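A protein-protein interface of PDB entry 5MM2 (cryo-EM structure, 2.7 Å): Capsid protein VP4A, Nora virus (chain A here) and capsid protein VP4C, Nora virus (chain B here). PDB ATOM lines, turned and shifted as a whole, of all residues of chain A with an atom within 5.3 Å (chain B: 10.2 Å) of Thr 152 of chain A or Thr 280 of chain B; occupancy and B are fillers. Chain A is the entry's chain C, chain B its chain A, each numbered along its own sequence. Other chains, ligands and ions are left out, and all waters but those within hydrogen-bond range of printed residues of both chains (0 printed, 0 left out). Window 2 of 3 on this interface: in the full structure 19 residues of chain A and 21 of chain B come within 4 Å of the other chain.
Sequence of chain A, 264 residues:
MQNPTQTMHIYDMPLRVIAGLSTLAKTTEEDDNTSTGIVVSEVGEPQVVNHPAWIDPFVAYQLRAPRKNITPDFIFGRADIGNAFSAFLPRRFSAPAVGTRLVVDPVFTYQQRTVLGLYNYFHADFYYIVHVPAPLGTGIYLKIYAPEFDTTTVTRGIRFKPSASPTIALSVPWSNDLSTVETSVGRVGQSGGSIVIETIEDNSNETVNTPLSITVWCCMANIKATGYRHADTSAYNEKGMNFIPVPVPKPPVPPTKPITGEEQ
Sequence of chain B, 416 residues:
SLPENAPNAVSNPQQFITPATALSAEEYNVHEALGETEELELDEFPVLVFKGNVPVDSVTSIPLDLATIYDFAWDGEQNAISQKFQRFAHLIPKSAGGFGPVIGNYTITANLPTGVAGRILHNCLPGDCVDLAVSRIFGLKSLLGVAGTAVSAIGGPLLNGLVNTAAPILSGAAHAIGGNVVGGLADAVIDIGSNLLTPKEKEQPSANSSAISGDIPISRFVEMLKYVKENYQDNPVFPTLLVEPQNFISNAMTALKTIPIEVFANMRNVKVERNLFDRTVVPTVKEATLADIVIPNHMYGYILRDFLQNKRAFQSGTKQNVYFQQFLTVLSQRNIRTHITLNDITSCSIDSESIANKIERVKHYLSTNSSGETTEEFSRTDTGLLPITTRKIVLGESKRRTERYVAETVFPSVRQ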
ATOM      1  N   ARG A 101      -7.457 -11.000  19.887  1.00  0.00           N
ATOM      2  CA  ARG A 101      -6.654 -10.616  18.740  1.00  0.00           C
ATOM      3  C   ARG A 101      -5.966  -9.287  19.027  1.00  0.00           C
ATOM      4  O   ARG A 101      -6.518  -8.429  19.715  1.00  0.00           O
ATOM      5  CB  ARG A 101      -7.532 -10.506  17.497  1.00  0.00           C
ATOM      6  CG  ARG A 101      -6.756 -10.581  16.250  1.00  0.00           C
ATOM      7  CD  ARG A 101      -7.581 -10.429  14.999  1.00  0.00           C
ATOM      8  NE  ARG A 101      -7.971  -9.053  14.744  1.00  0.00           N
ATOM      9  CZ  ARG A 101      -8.574  -8.662  13.630  1.00  0.00           C
ATOM     10  NH1 ARG A 101      -8.831  -9.548  12.678  1.00  0.00           N
ATOM     11  NH2 ARG A 101      -8.913  -7.394  13.458  1.00  0.00           N
ATOM     12  N   ASP A 150     -12.402  -6.626   8.160  1.00  0.00           N
ATOM     13  CA  ASP A 150     -13.072  -6.494   9.439  1.00  0.00           C
ATOM     14  C   ASP A 150     -12.331  -7.283  10.512  1.00  0.00           C
ATOM     15  O   ASP A 150     -11.167  -7.639  10.359  1.00  0.00           O
ATOM     16  CB  ASP A 150     -14.532  -6.914   9.295  1.00  0.00           C
ATOM     17  CG  ASP A 150     -14.690  -8.293   8.703  1.00  0.00           C
ATOM     18  OD1 ASP A 150     -13.686  -8.939   8.356  1.00  0.00           O
ATOM     19  OD2 ASP A 150     -15.841  -8.724   8.543  1.00  0.00           O
ATOM     20  N   THR A 151     -13.025  -7.540  11.610  1.00  0.00           N
ATOM     21  CA  THR A 151     -12.440  -8.097  12.818  1.00  0.00           C
ATOM     22  C   THR A 151     -12.143  -9.591  12.717  1.00  0.00           C
ATOM     23  O   THR A 151     -11.224 -10.073  13.379  1.00  0.00           O
ATOM     24  CB  THR A 151     -13.399  -7.791  13.970  1.00  0.00           C
ATOM     25  OG1 THR A 151     -13.692  -6.392  13.950  1.00  0.00           O
ATOM     26  CG2 THR A 151     -12.792  -8.106  15.326  1.00  0.00           C
ATOM     27  N   THR A 152     -12.853 -10.349  11.900  1.00  0.00           N
ATOM     28  CA  THR A 152     -12.667 -11.788  11.928  1.00  0.00           C
ATOM     29  C   THR A 152     -11.918 -12.364  10.739  1.00  0.00           C
ATOM     30  O   THR A 152     -11.626 -13.562  10.751  1.00  0.00           O
ATOM     31  CB  THR A 152     -14.020 -12.500  12.048  1.00  0.00           C
ATOM     32  OG1 THR A 152     -14.838 -12.172  10.922  1.00  0.00           O
ATOM     33  CG2 THR A 152     -14.721 -12.065  13.309  1.00  0.00           C
ATOM     34  N   THR A 153     -11.578 -11.565   9.739  1.00  0.00           N
ATOM     35  CA  THR A 153     -11.067 -12.096   8.483  1.00  0.00           C
ATOM     36  C   THR A 153      -9.602 -12.496   8.618  1.00  0.00           C
ATOM     37  O   THR A 153      -8.781 -11.711   9.096  1.00  0.00           O
ATOM     38  CB  THR A 153     -11.240 -11.056   7.385  1.00  0.00           C
ATOM     39  OG1 THR A 153     -12.620 -10.697   7.296  1.00  0.00           O
ATOM     40  CG2 THR A 153     -10.801 -11.602   6.061  1.00  0.00           C
ATOM     41  N   VAL A 154      -9.280 -13.717   8.199  1.00  0.00           N
ATOM     42  CA  VAL A 154      -7.946 -14.290   8.337  1.00  0.00           C
ATOM     43  C   VAL A 154      -7.371 -14.500   6.946  1.00  0.00           C
ATOM     44  O   VAL A 154      -8.070 -14.985   6.054  1.00  0.00           O
ATOM     45  CB  VAL A 154      -7.997 -15.618   9.111  1.00  0.00           C
ATOM     46  CG1 VAL A 154      -6.617 -16.203   9.299  1.00  0.00           C
ATOM     47  CG2 VAL A 154      -8.676 -15.425  10.438  1.00  0.00           C
ATOM     48  N   GLN B  86     -16.896 -13.296  -3.075  1.00  0.00           N
ATOM     49  CA  GLN B  86     -16.826 -13.828  -1.722  1.00  0.00           C
ATOM     50  C   GLN B  86     -15.409 -14.250  -1.378  1.00  0.00           C
ATOM     51  O   GLN B  86     -14.907 -13.940  -0.295  1.00  0.00           O
ATOM     52  CB  GLN B  86     -17.765 -15.017  -1.582  1.00  0.00           C
ATOM     53  CG  GLN B  86     -19.223 -14.700  -1.750  1.00  0.00           C
ATOM     54  CD  GLN B  86     -19.767 -13.901  -0.608  1.00  0.00           C
ATOM     55  OE1 GLN B  86     -19.423 -14.137   0.543  1.00  0.00           O
ATOM     56  NE2 GLN B  86     -20.621 -12.939  -0.914  1.00  0.00           N
ATOM     57  N   ASN B 275      -6.813 -13.934  -1.012  1.00  0.00           N
ATOM     58  CA  ASN B 275      -7.826 -14.929  -0.689  1.00  0.00           C
ATOM     59  C   ASN B 275      -8.218 -14.830   0.782  1.00  0.00           C
ATOM     60  O   ASN B 275      -7.353 -14.817   1.657  1.00  0.00           O
ATOM     61  CB  ASN B 275      -7.259 -16.308  -1.014  1.00  0.00           C
ATOM     62  CG  ASN B 275      -8.307 -17.377  -1.082  1.00  0.00           C
ATOM     63  OD1 ASN B 275      -9.488 -17.121  -0.897  1.00  0.00           O
ATOM     64  ND2 ASN B 275      -7.882 -18.596  -1.362  1.00  0.00           N
ATOM     65  N   LEU B 276      -9.517 -14.763   1.064  1.00  0.00           N
ATOM     66  CA  LEU B 276     -10.014 -14.417   2.391  1.00  0.00           C
ATOM     67  C   LEU B 276     -10.746 -15.577   3.048  1.00  0.00           C
ATOM     68  O   LEU B 276     -11.501 -16.297   2.395  1.00  0.00           O
ATOM     69  CB  LEU B 276     -10.961 -13.231   2.314  1.00  0.00           C
ATOM     70  CG  LEU B 276     -10.320 -11.988   1.734  1.00  0.00           C
ATOM     71  CD1 LEU B 276     -11.343 -10.924   1.652  1.00  0.00           C
ATOM     72  CD2 LEU B 276      -9.174 -11.548   2.587  1.00  0.00           C
ATOM     73  N   PHE B 277     -10.563 -15.716   4.357  1.00  0.00           N
ATOM     74  CA  PHE B 277     -11.122 -16.817   5.123  1.00  0.00           C
ATOM     75  C   PHE B 277     -11.946 -16.270   6.274  1.00  0.00           C
ATOM     76  O   PHE B 277     -11.693 -15.163   6.749  1.00  0.00           O
ATOM     77  CB  PHE B 277     -10.019 -17.730   5.642  1.00  0.00           C
ATOM     78  CG  PHE B 277      -9.363 -18.527   4.570  1.00  0.00           C
ATOM     79  CD1 PHE B 277      -9.847 -19.771   4.238  1.00  0.00           C
ATOM     80  CD2 PHE B 277      -8.318 -18.002   3.836  1.00  0.00           C
ATOM     81  CE1 PHE B 277      -9.267 -20.500   3.239  1.00  0.00           C
ATOM     82  CE2 PHE B 277      -7.744 -18.721   2.827  1.00  0.00           C
ATOM     83  CZ  PHE B 277      -8.222 -19.974   2.530  1.00  0.00           C
ATOM     84  N   ASP B 278     -12.982 -17.038   6.637  1.00  0.00           N
ATOM     85  CA  ASP B 278     -14.002 -16.856   7.679  1.00  0.00           C
ATOM     86  C   ASP B 278     -14.394 -15.405   7.955  1.00  0.00           C
ATOM     87  O   ASP B 278     -14.464 -14.969   9.104  1.00  0.00           O
ATOM     88  CB  ASP B 278     -13.632 -17.624   8.971  1.00  0.00           C
ATOM     89  CG  ASP B 278     -12.373 -17.138   9.677  1.00  0.00           C
ATOM     90  OD1 ASP B 278     -11.785 -16.105   9.346  1.00  0.00           O
ATOM     91  OD2 ASP B 278     -11.951 -17.843  10.613  1.00  0.00           O
ATOM     92  N   ARG B 279     -14.689 -14.670   6.892  1.00  0.00           N
ATOM     93  CA  ARG B 279     -15.020 -13.260   6.983  1.00  0.00           C
ATOM     94  C   ARG B 279     -16.445 -13.067   7.480  1.00  0.00           C
ATOM     95  O   ARG B 279     -17.289 -13.956   7.390  1.00  0.00           O
ATOM     96  CB  ARG B 279     -14.826 -12.598   5.623  1.00  0.00           C
ATOM     97  CG  ARG B 279     -15.657 -13.201   4.549  1.00  0.00           C
ATOM     98  CD  ARG B 279     -15.301 -12.657   3.192  1.00  0.00           C
ATOM     99  NE  ARG B 279     -15.656 -11.260   3.022  1.00  0.00           N
ATOM    100  CZ  ARG B 279     -15.333 -10.553   1.951  1.00  0.00           C
ATOM    101  NH1 ARG B 279     -14.671 -11.124   0.967  1.00  0.00           N
ATOM    102  NH2 ARG B 279     -15.689  -9.287   1.850  1.00  0.00           N
ATOM    103  N   THR B 280     -16.705 -11.878   8.017  1.00  0.00           N
ATOM    104  CA  THR B 280     -18.002 -11.531   8.578  1.00  0.00           C
ATOM    105  C   THR B 280     -18.796 -10.594   7.679  1.00  0.00           C
ATOM    106  O   THR B 280     -19.969 -10.855   7.394  1.00  0.00           O
ATOM    107  CB  THR B 280     -17.818 -10.894   9.959  1.00  0.00           C
ATOM    108  OG1 THR B 280     -17.163 -11.825  10.827  1.00  0.00           O
ATOM    109  CG2 THR B 280     -19.150 -10.508  10.558  1.00  0.00           C
ATOM    110  N   VAL B 281     -18.186  -9.511   7.219  1.00  0.00           N
ATOM    111  CA  VAL B 281     -18.842  -8.579   6.310  1.00  0.00           C
ATOM    112  C   VAL B 281     -18.637  -9.091   4.890  1.00  0.00           C
ATOM    113  O   VAL B 281     -17.525  -9.054   4.363  1.00  0.00           O
ATOM    114  CB  VAL B 281     -18.300  -7.157   6.475  1.00  0.00           C
ATOM    115  CG1 VAL B 281     -18.961  -6.232   5.481  1.00  0.00           C
ATOM    116  CG2 VAL B 281     -18.526  -6.674   7.889  1.00  0.00           C
ATOM    117  N   VAL B 282     -19.713  -9.562   4.273  1.00  0.00           N
ATOM    118  CA  VAL B 282     -19.687 -10.161   2.942  1.00  0.00           C
ATOM    119  C   VAL B 282     -20.391  -9.200   1.989  1.00  0.00           C
ATOM    120  O   VAL B 282     -21.053  -8.266   2.458  1.00  0.00           O
ATOM    121  CB  VAL B 282     -20.338 -11.551   2.973  1.00  0.00           C
ATOM    122  CG1 VAL B 282     -19.543 -12.462   3.869  1.00  0.00           C
ATOM    123  CG2 VAL B 282     -21.758 -11.445   3.463  1.00  0.00           C
ATOM    124  N   PRO B 283     -20.271  -9.351   0.665  1.00  0.00           N
ATOM    125  CA  PRO B 283     -20.977  -8.436  -0.245  1.00  0.00           C
ATOM    126  C   PRO B 283     -22.485  -8.627  -0.364  1.00  0.00           C
ATOM    127  O   PRO B 283     -23.067  -7.967  -1.227  1.00  0.00           O
ATOM    128  CB  PRO B 283     -20.300  -8.697  -1.592  1.00  0.00           C
ATOM    129  CG  PRO B 283     -18.975  -9.152  -1.247  1.00  0.00           C
ATOM    130  CD  PRO B 283     -19.123  -9.972  -0.019  1.00  0.00           C
ATOM    131  N   THR B 284     -23.139  -9.463   0.462  1.00  0.00           N
ATOM    132  CA  THR B 284     -24.599  -9.576   0.668  1.00  0.00           C
ATOM    133  C   THR B 284     -25.488  -9.548  -0.586  1.00  0.00           C
ATOM    134  O   THR B 284     -26.149  -8.545  -0.869  1.00  0.00           O
ATOM    135  CB  THR B 284     -25.131  -8.567   1.729  1.00  0.00           C
ATOM    136  OG1 THR B 284     -26.552  -8.706   1.844  1.00  0.00           O
ATOM    137  CG2 THR B 284     -24.756  -7.059   1.550  1.00  0.00           C
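Thr 152 of chain A touches Arg 279 of chain B.
CD2 of Leu 276 of chain B touches CG2 of Thr 153 of chain A, 3.8 Å away.
CA of Thr 153 of chain A touches O of Phe 277 of chain B, 3.6 Å away.
OG1 of Thr 153 of chain A touches CB of Arg 279 of chain B (3.4 Å).
Val 154 of chain A touches Asp 278 of chain B.
N of Phe 277 of chain B is in hydrogen-bond range of O of Val 154 of chain A.
N of Thr 280 of chain B sits close to OD2 of Asp 150 of chain A (3.3 Å).
The side-chain carboxylate of Asp 150 of chain A lies within hydrogen-bond range of the backbone NH of Val 281 of chain B, at 2.8 Å.
N of Thr 280 of chain B sits close to OG1 of Thr 152 of chain A (3.5 Å).
The backbone carbonyl oxygen (O) of Asp 278 of chain B is in hydrogen-bond range of the side-chain hydroxyl (OG1) of Thr 152 of chain A (3.4 Å).
Printed residues of chain B that touch a printed residue of chain A: Leu 276, Phe 277, Asp 278, Arg 279, Thr 280 and Val 281.
Hydrophobic or aromatic side chains of chain B that line the printed part of chain A: Leu 276, Phe 277 and Val 281.
Among the printed residues, no Asp or Glu carboxylate lies within 4 Å of a Lys or Arg side-chain nitrogen of the other chain.
The guanidinium group of Arg 279 of chain B sits at hydrogen-bond distance from the backbone carbonyl oxygen of Val 281 of chain B (3.1 Å).
The guanidinium group (NH1) of Arg 279 of chain B sits at hydrogen-bond distance from the backbone carbonyl oxygen (O) of Gln 86 of chain B (3.1 Å).
No residue of chain B comes within 4 Å of Thr 151 of chain A.
Of chain B, only Asp 278, Arg 279 and Thr 280 come within 4 Å of Thr 152 of chain A.
Asn 275 of chain B touches none of the printed residues of chain A.
Of the printed residues of chain A, Phe 277 of chain B touches Thr 153 (3.6 Å) and Val 154 (3.1 Å).
Printed residues of chain A within 4 Å of Asp 278 of chain B: Thr 152 (2.9 Å) and Val 154 (3.4 Å).
Pro 283 of chain B touches none of the printed residues of chain A.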
